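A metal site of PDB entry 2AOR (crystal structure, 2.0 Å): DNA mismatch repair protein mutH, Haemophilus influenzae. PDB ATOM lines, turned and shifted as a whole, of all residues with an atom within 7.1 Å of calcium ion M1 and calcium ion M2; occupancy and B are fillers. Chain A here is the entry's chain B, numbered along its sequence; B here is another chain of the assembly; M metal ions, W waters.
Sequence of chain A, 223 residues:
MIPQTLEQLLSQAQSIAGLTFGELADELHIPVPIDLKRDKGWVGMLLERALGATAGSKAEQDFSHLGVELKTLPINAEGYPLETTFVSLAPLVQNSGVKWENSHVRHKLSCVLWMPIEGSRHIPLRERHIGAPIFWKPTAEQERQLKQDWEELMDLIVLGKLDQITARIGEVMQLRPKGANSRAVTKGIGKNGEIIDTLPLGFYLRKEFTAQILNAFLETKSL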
ATOM      1  N   GLY A  44      -6.789 -17.911 -18.219  1.00  0.00           N
ATOM      2  CA  GLY A  44      -5.809 -18.974 -18.253  1.00  0.00           C
ATOM      3  C   GLY A  44      -5.613 -19.621 -16.885  1.00  0.00           C
ATOM      4  O   GLY A  44      -5.425 -20.834 -16.783  1.00  0.00           O
ATOM      5  N   MET A  45      -5.650 -18.804 -15.827  1.00  0.00           N
ATOM      6  CA  MET A  45      -5.479 -19.335 -14.477  1.00  0.00           C
ATOM      7  C   MET A  45      -6.719 -20.104 -14.096  1.00  0.00           C
ATOM      8  O   MET A  45      -6.646 -21.124 -13.398  1.00  0.00           O
ATOM      9  CB  MET A  45      -5.253 -18.215 -13.442  1.00  0.00           C
ATOM     10  CG  MET A  45      -4.165 -17.235 -13.811  1.00  0.00           C
ATOM     11  SD  MET A  45      -2.560 -17.984 -14.198  1.00  0.00           S
ATOM     12  CE  MET A  45      -1.506 -16.504 -14.201  1.00  0.00           C
ATOM     13  N   GLU A  48      -6.525 -23.527 -15.455  1.00  0.00           N
ATOM     14  CA  GLU A  48      -5.502 -24.322 -14.776  1.00  0.00           C
ATOM     15  C   GLU A  48      -6.098 -24.891 -13.486  1.00  0.00           C
ATOM     16  O   GLU A  48      -5.881 -26.055 -13.162  1.00  0.00           O
ATOM     17  CB  GLU A  48      -4.265 -23.477 -14.437  1.00  0.00           C
ATOM     18  CG  GLU A  48      -3.429 -23.113 -15.645  1.00  0.00           C
ATOM     19  CD  GLU A  48      -2.195 -22.290 -15.301  1.00  0.00           C
ATOM     20  OE1 GLU A  48      -2.182 -21.597 -14.257  1.00  0.00           O
ATOM     21  OE2 GLU A  48      -1.221 -22.314 -16.088  1.00  0.00           O
ATOM     22  N   ALA A  53      -3.925 -28.130 -13.025  1.00  0.00           N
ATOM     23  CA  ALA A  53      -2.561 -27.716 -13.315  1.00  0.00           C
ATOM     24  C   ALA A  53      -2.168 -26.911 -12.071  1.00  0.00           C
ATOM     25  O   ALA A  53      -3.032 -26.569 -11.263  1.00  0.00           O
ATOM     26  CB  ALA A  53      -2.537 -26.833 -14.555  1.00  0.00           C
ATOM     27  N   THR A  54      -0.892 -26.596 -11.907  1.00  0.00           N
ATOM     28  CA  THR A  54      -0.487 -25.833 -10.728  1.00  0.00           C
ATOM     29  C   THR A  54      -0.215 -24.357 -10.990  1.00  0.00           C
ATOM     30  O   THR A  54       0.479 -23.991 -11.947  1.00  0.00           O
ATOM     31  CB  THR A  54       0.739 -26.474 -10.054  1.00  0.00           C
ATOM     32  OG1 THR A  54       1.770 -26.677 -11.037  1.00  0.00           O
ATOM     33  CG2 THR A  54       0.373 -27.808  -9.430  1.00  0.00           C
ATOM     34  N   ALA A  55      -0.776 -23.506 -10.135  1.00  0.00           N
ATOM     35  CA  ALA A  55      -0.602 -22.064 -10.258  1.00  0.00           C
ATOM     36  C   ALA A  55       0.839 -21.631  -9.988  1.00  0.00           C
ATOM     37  O   ALA A  55       1.499 -22.163  -9.101  1.00  0.00           O
ATOM     38  CB  ALA A  55      -1.554 -21.345  -9.306  1.00  0.00           C
ATOM     39  N   GLY A  56       1.324 -20.664 -10.772  1.00  0.00           N
ATOM     40  CA  GLY A  56       2.673 -20.160 -10.605  1.00  0.00           C
ATOM     41  C   GLY A  56       3.753 -21.046 -11.188  1.00  0.00           C
ATOM     42  O   GLY A  56       4.827 -20.567 -11.536  1.00  0.00           O
ATOM     43  N   SER A  57       3.470 -22.347 -11.293  1.00  0.00           N
ATOM     44  CA  SER A  57       4.417 -23.323 -11.825  1.00  0.00           C
ATOM     45  C   SER A  57       5.221 -22.849 -13.048  1.00  0.00           C
ATOM     46  O   SER A  57       4.705 -22.146 -13.917  1.00  0.00           O
ATOM     47  CB  SER A  57       3.694 -24.633 -12.174  1.00  0.00           C
ATOM     48  OG  SER A  57       4.604 -25.586 -12.715  1.00  0.00           O
ATOM     49  N   LYS A  58       6.488 -23.260 -13.095  1.00  0.00           N
ATOM     50  CA  LYS A  58       7.371 -22.883 -14.182  1.00  0.00           C
ATOM     51  C   LYS A  58       7.911 -24.131 -14.897  1.00  0.00           C
ATOM     52  O   LYS A  58       8.985 -24.088 -15.507  1.00  0.00           O
ATOM     53  CB  LYS A  58       8.554 -22.066 -13.626  1.00  0.00           C
ATOM     54  CG  LYS A  58       8.194 -21.111 -12.501  1.00  0.00           C
ATOM     55  CD  LYS A  58       8.231 -19.649 -12.955  1.00  0.00           C
ATOM     56  CE  LYS A  58       6.985 -19.253 -13.746  1.00  0.00           C
ATOM     57  NZ  LYS A  58       5.919 -18.645 -12.891  1.00  0.00           N
ATOM     58  N   ALA A  59       7.170 -25.235 -14.829  1.00  0.00           N
ATOM     59  CA  ALA A  59       7.573 -26.471 -15.484  1.00  0.00           C
ATOM     60  C   ALA A  59       7.413 -26.307 -16.990  1.00  0.00           C
ATOM     61  O   ALA A  59       6.613 -25.495 -17.439  1.00  0.00           O
ATOM     62  CB  ALA A  59       6.719 -27.631 -14.992  1.00  0.00           C
ATOM     63  N   GLU A  60       8.155 -27.085 -17.783  1.00  0.00           N
ATOM     64  CA  GLU A  60       8.070 -26.977 -19.236  1.00  0.00           C
ATOM     65  C   GLU A  60       6.652 -27.194 -19.795  1.00  0.00           C
ATOM     66  O   GLU A  60       6.218 -26.469 -20.682  1.00  0.00           O
ATOM     67  CB  GLU A  60       9.048 -27.949 -19.903  1.00  0.00           C
ATOM     68  CG  GLU A  60       9.292 -27.666 -21.377  1.00  0.00           C
ATOM     69  CD  GLU A  60      10.586 -26.892 -21.639  1.00  0.00           C
ATOM     70  OE1 GLU A  60      10.676 -25.712 -21.228  1.00  0.00           O
ATOM     71  OE2 GLU A  60      11.509 -27.465 -22.258  1.00  0.00           O
ATOM     72  N   GLN A  61       5.943 -28.197 -19.282  1.00  0.00           N
ATOM     73  CA  GLN A  61       4.572 -28.491 -19.683  1.00  0.00           C
ATOM     74  C   GLN A  61       3.684 -28.465 -18.437  1.00  0.00           C
ATOM     75  O   GLN A  61       4.136 -28.837 -17.350  1.00  0.00           O
ATOM     76  CB  GLN A  61       4.448 -29.879 -20.322  1.00  0.00           C
ATOM     77  CG  GLN A  61       5.145 -30.075 -21.654  1.00  0.00           C
ATOM     78  CD  GLN A  61       5.160 -31.531 -22.089  1.00  0.00           C
ATOM     79  OE1 GLN A  61       5.536 -32.405 -21.318  1.00  0.00           O
ATOM     80  NE2 GLN A  61       4.745 -31.793 -23.323  1.00  0.00           N
ATOM     81  N   ASP A  62       2.440 -28.036 -18.592  1.00  0.00           N
ATOM     82  CA  ASP A  62       1.511 -27.964 -17.479  1.00  0.00           C
ATOM     83  C   ASP A  62       1.321 -29.330 -16.818  1.00  0.00           C
ATOM     84  O   ASP A  62       1.224 -29.436 -15.605  1.00  0.00           O
ATOM     85  CB  ASP A  62       0.164 -27.433 -17.959  1.00  0.00           C
ATOM     86  CG  ASP A  62       0.267 -26.013 -18.480  1.00  0.00           C
ATOM     87  OD1 ASP A  62       0.677 -25.140 -17.697  1.00  0.00           O
ATOM     88  OD2 ASP A  62      -0.041 -25.769 -19.666  1.00  0.00           O
ATOM     89  N   VAL A  68       1.497 -33.114 -21.566  1.00  0.00           N
ATOM     90  CA  VAL A  68       0.502 -32.203 -22.132  1.00  0.00           C
ATOM     91  C   VAL A  68       0.663 -30.758 -21.675  1.00  0.00           C
ATOM     92  O   VAL A  68       0.946 -30.484 -20.505  1.00  0.00           O
ATOM     93  CB  VAL A  68      -0.930 -32.660 -21.760  1.00  0.00           C
ATOM     94  CG1 VAL A  68      -1.962 -31.677 -22.344  1.00  0.00           C
ATOM     95  CG2 VAL A  68      -1.164 -34.082 -22.255  1.00  0.00           C
ATOM     96  N   GLU A  69       0.461 -29.821 -22.600  1.00  0.00           N
ATOM     97  CA  GLU A  69       0.534 -28.390 -22.300  1.00  0.00           C
ATOM     98  C   GLU A  69      -0.888 -27.831 -22.430  1.00  0.00           C
ATOM     99  O   GLU A  69      -1.578 -28.101 -23.417  1.00  0.00           O
ATOM    100  CB  GLU A  69       1.467 -27.667 -23.289  1.00  0.00           C
ATOM    101  CG  GLU A  69       1.322 -26.142 -23.262  1.00  0.00           C
ATOM    102  CD  GLU A  69       1.855 -25.507 -21.964  1.00  0.00           C
ATOM    103  OE1 GLU A  69       1.552 -24.309 -21.724  1.00  0.00           O
ATOM    104  OE2 GLU A  69       2.578 -26.188 -21.202  1.00  0.00           O
ATOM    105  N   LEU A  70      -1.320 -27.044 -21.456  1.00  0.00           N
ATOM    106  CA  LEU A  70      -2.662 -26.458 -21.493  1.00  0.00           C
ATOM    107  C   LEU A  70      -2.593 -25.010 -21.981  1.00  0.00           C
ATOM    108  O   LEU A  70      -1.753 -24.239 -21.518  1.00  0.00           O
ATOM    109  CB  LEU A  70      -3.294 -26.505 -20.095  1.00  0.00           C
ATOM    110  CG  LEU A  70      -4.582 -25.707 -19.892  1.00  0.00           C
ATOM    111  CD1 LEU A  70      -5.719 -26.332 -20.721  1.00  0.00           C
ATOM    112  CD2 LEU A  70      -4.952 -25.675 -18.402  1.00  0.00           C
ATOM    113  N   LYS A  71      -3.447 -24.659 -22.929  1.00  0.00           N
ATOM    114  CA  LYS A  71      -3.473 -23.291 -23.450  1.00  0.00           C
ATOM    115  C   LYS A  71      -4.896 -22.842 -23.805  1.00  0.00           C
ATOM    116  O   LYS A  71      -5.589 -23.518 -24.559  1.00  0.00           O
ATOM    117  CB  LYS A  71      -2.604 -23.165 -24.712  1.00  0.00           C
ATOM    118  CG  LYS A  71      -1.227 -23.826 -24.612  1.00  0.00           C
ATOM    119  CD  LYS A  71      -0.330 -23.373 -25.740  1.00  0.00           C
ATOM    120  CE  LYS A  71       0.583 -22.236 -25.293  1.00  0.00           C
ATOM    121  NZ  LYS A  71       1.780 -22.736 -24.540  1.00  0.00           N
ATOM    122  N   THR A  72      -5.331 -21.720 -23.238  1.00  0.00           N
ATOM    123  CA  THR A  72      -6.638 -21.193 -23.614  1.00  0.00           C
ATOM    124  C   THR A  72      -6.415 -20.450 -24.920  1.00  0.00           C
ATOM    125  O   THR A  72      -5.304 -19.959 -25.187  1.00  0.00           O
ATOM    126  CB  THR A  72      -7.203 -20.203 -22.591  1.00  0.00           C
ATOM    127  OG1 THR A  72      -6.300 -19.099 -22.443  1.00  0.00           O
ATOM    128  CG2 THR A  72      -7.432 -20.892 -21.236  1.00  0.00           C
ATOM    129  N   LYS A 108       7.047 -27.737 -25.809  1.00  0.00           N
ATOM    130  CA  LYS A 108       5.774 -27.181 -25.396  1.00  0.00           C
ATOM    131  C   LYS A 108       4.648 -27.399 -26.385  1.00  0.00           C
ATOM    132  O   LYS A 108       3.495 -27.567 -25.986  1.00  0.00           O
ATOM    133  CB  LYS A 108       5.931 -25.677 -25.123  1.00  0.00           C
ATOM    134  CG  LYS A 108       6.583 -25.382 -23.791  1.00  0.00           C
ATOM    135  CD  LYS A 108       7.022 -23.939 -23.679  1.00  0.00           C
ATOM    136  CE  LYS A 108       7.299 -23.565 -22.235  1.00  0.00           C
ATOM    137  NZ  LYS A 108       6.037 -23.698 -21.439  1.00  0.00           N
ATOM    138  P    DG B  15       8.738 -19.816 -17.984  1.00  0.00           P
ATOM    139  OP1  DG B  15       9.182 -21.233 -17.886  1.00  0.00           O
ATOM    140  OP2  DG B  15       9.151 -18.999 -19.154  1.00  0.00           O
ATOM    141  O5'  DG B  15       7.162 -19.780 -17.860  1.00  0.00           O
ATOM    142  C5'  DG B  15       6.557 -20.315 -16.704  1.00  0.00           C
ATOM    143  C4'  DG B  15       5.092 -19.952 -16.672  1.00  0.00           C
ATOM    144  O4'  DG B  15       4.920 -18.575 -16.254  1.00  0.00           O
ATOM    145  C3'  DG B  15       4.421 -20.087 -18.034  1.00  0.00           C
ATOM    146  O3'  DG B  15       3.184 -20.764 -17.869  1.00  0.00           O
ATOM    147  C2'  DG B  15       4.192 -18.651 -18.475  1.00  0.00           C
ATOM    148  C1'  DG B  15       4.036 -17.921 -17.149  1.00  0.00           C
ATOM    149  N9   DG B  15       4.389 -16.506 -17.194  1.00  0.00           N
ATOM    150  C8   DG B  15       5.438 -15.938 -17.889  1.00  0.00           C
ATOM    151  N7   DG B  15       5.468 -14.641 -17.791  1.00  0.00           N
ATOM    152  C5   DG B  15       4.392 -14.325 -16.973  1.00  0.00           C
ATOM    153  C6   DG B  15       3.931 -13.081 -16.526  1.00  0.00           C
ATOM    154  O6   DG B  15       4.387 -11.966 -16.756  1.00  0.00           O
ATOM    155  N1   DG B  15       2.808 -13.202 -15.715  1.00  0.00           N
ATOM    156  C2   DG B  15       2.224 -14.393 -15.371  1.00  0.00           C
ATOM    157  N2   DG B  15       1.156 -14.308 -14.575  1.00  0.00           N
ATOM    158  N3   DG B  15       2.646 -15.581 -15.789  1.00  0.00           N
ATOM    159  C4   DG B  15       3.732 -15.463 -16.582  1.00  0.00           C
ATOM    160  P    DG B  16       2.223 -20.954 -19.124  1.00  0.00           P
ATOM    161  OP1  DG B  16       1.636 -22.310 -18.984  1.00  0.00           O
ATOM    162  OP2  DG B  16       2.960 -20.588 -20.344  1.00  0.00           O
ATOM    163  O5'  DG B  16       1.080 -19.874 -18.865  1.00  0.00           O
ATOM    164  C5'  DG B  16       0.167 -20.062 -17.795  1.00  0.00           C
ATOM    165  C4'  DG B  16      -0.759 -18.886 -17.693  1.00  0.00           C
ATOM    166  O4'  DG B  16      -0.050 -17.718 -17.192  1.00  0.00           O
ATOM    167  C3'  DG B  16      -1.360 -18.390 -19.000  1.00  0.00           C
ATOM    168  O3'  DG B  16      -2.421 -19.236 -19.429  1.00  0.00           O
ATOM    169  C2'  DG B  16      -1.832 -17.003 -18.604  1.00  0.00           C
ATOM    170  C1'  DG B  16      -0.702 -16.546 -17.666  1.00  0.00           C
ATOM    171  N9   DG B  16       0.262 -15.675 -18.306  1.00  0.00           N
ATOM    172  C8   DG B  16       1.285 -16.024 -19.161  1.00  0.00           C
ATOM    173  N7   DG B  16       1.949 -14.999 -19.614  1.00  0.00           N
ATOM    174  C5   DG B  16       1.344 -13.894 -19.013  1.00  0.00           C
ATOM    175  C6   DG B  16       1.633 -12.499 -19.114  1.00  0.00           C
ATOM    176  O6   DG B  16       2.514 -11.933 -19.766  1.00  0.00           O
ATOM    177  N1   DG B  16       0.756 -11.746 -18.334  1.00  0.00           N
ATOM    178  C2   DG B  16      -0.247 -12.242 -17.561  1.00  0.00           C
ATOM    179  N2   DG B  16      -0.976 -11.347 -16.892  1.00  0.00           N
ATOM    180  N3   DG B  16      -0.521 -13.542 -17.460  1.00  0.00           N
ATOM    181  C4   DG B  16       0.310 -14.297 -18.207  1.00  0.00           C
ATOM    182  P    DA B  17      -2.896 -19.186 -20.963  1.00  0.00           P
ATOM    183  OP1  DA B  17      -4.045 -20.137 -21.058  1.00  0.00           O
ATOM    184  OP2  DA B  17      -1.719 -19.382 -21.846  1.00  0.00           O
ATOM    185  O5'  DA B  17      -3.452 -17.700 -21.088  1.00  0.00           O
ATOM    186  C5'  DA B  17      -3.234 -16.877 -22.239  1.00  0.00           C
ATOM    187  C4'  DA B  17      -3.327 -15.426 -21.823  1.00  0.00           C
ATOM    188  O4'  DA B  17      -2.013 -14.951 -21.414  1.00  0.00           O
ATOM    189  C3'  DA B  17      -3.781 -14.378 -22.820  1.00  0.00           C
ATOM    190  O3'  DA B  17      -5.207 -14.367 -22.848  1.00  0.00           O
ATOM    191  C2'  DA B  17      -3.263 -13.084 -22.188  1.00  0.00           C
ATOM    192  C1'  DA B  17      -1.986 -13.537 -21.490  1.00  0.00           C
ATOM    193  N9   DA B  17      -0.764 -13.118 -22.171  1.00  0.00           N
ATOM    194  C8   DA B  17       0.063 -13.838 -22.989  1.00  0.00           C
ATOM    195  N7   DA B  17       1.059 -13.140 -23.471  1.00  0.00           N
ATOM    196  C5   DA B  17       0.903 -11.883 -22.919  1.00  0.00           C
ATOM    197  C6   DA B  17       1.648 -10.688 -23.014  1.00  0.00           C
ATOM    198  N6   DA B  17       2.773 -10.565 -23.737  1.00  0.00           N
ATOM    199  N1   DA B  17       1.198  -9.605 -22.335  1.00  0.00           N
ATOM    200  C2   DA B  17       0.089  -9.732 -21.596  1.00  0.00           C
ATOM    201  N3   DA B  17      -0.684 -10.800 -21.421  1.00  0.00           N
ATOM    202  C4   DA B  17      -0.224 -11.854 -22.109  1.00  0.00           C
HETATM  203 CA    CA M   1       0.058 -23.549 -20.281  1.00  0.00          CA
HETATM  204 CA    CA M   2       1.098 -23.059 -16.075  1.00  0.00          CA
HETATM  205  O   HOH W   1       2.930 -23.758 -17.213  1.00  0.00           O
HETATM  206  O   HOH W   2       0.625 -25.076 -14.661  1.00  0.00           O
HETATM  207  O   HOH W   3      -1.716 -23.027 -18.708  1.00  0.00           O
HETATM  208  O   HOH W   4       1.972 -21.555 -14.617  1.00  0.00           O
HETATM  209  O   HOH W   5      -0.156 -21.686 -21.518  1.00  0.00           O
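Water W1 binds calcium ion M2, at 2.3 Å.
Calcium ion M2 is bound by water W4 (2.3 Å).
Calcium ion M2 is bound by the side-chain carboxylate (OE2) of Glu 48, at 2.4 Å.
Water W2 binds calcium ion M2 (2.5 Å).
Calcium ion M2 is bound by the side-chain carboxylate (OD1) of Asp 62 (2.7 Å).
Calcium ion M2 has five donor atoms within binding distance.
Slightly farther from calcium ion M2 lies OP1 of DG 16 of chain B (3.1 Å).
Of the 22 residues printed, 4 come within 4 Å of calcium ion M1.
Along chain A the residues within 4 Å of calcium ion M1 span positions 62 to 70.
Residues that only touch calcium ion M2: DG 15 of chain B.
Within 4 Å of calcium ion M2: Glu 48, Asp 62, DG 15 of chain B and DG 16 of chain B.
Along chain A the residues within 4 Å of calcium ion M2 span positions 48 to 62.
N of Asp 62 lies within hydrogen-bond range of O of Val 68 (3.4 Å).
The backbone NH of Ala 53 is in hydrogen-bond range of the backbone carbonyl oxygen of Glu 48, at 2.9 Å.
The side-chain carboxylate (OE1) of Glu 69 sits close to the side-chain amino group (NZ) of Lys 71 (3.2 Å).
Calcium ion M1 is bound by the side-chain carboxylate (OE1) of Glu 69 (2.2 Å).
Water W5 is bound to calcium ion M1, at 2.2 Å.
O of Leu 70 binds calcium ion M1, at 2.3 Å.
OD2 of Asp 62 binds calcium ion M1 (2.3 Å).
Calcium ion M1 is bound by OP1 of DG 16 of chain B.
Water W3 is bound to calcium ion M1.
Slightly farther from calcium ion M1 lies OD1 of Asp 62 (3.1 Å).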
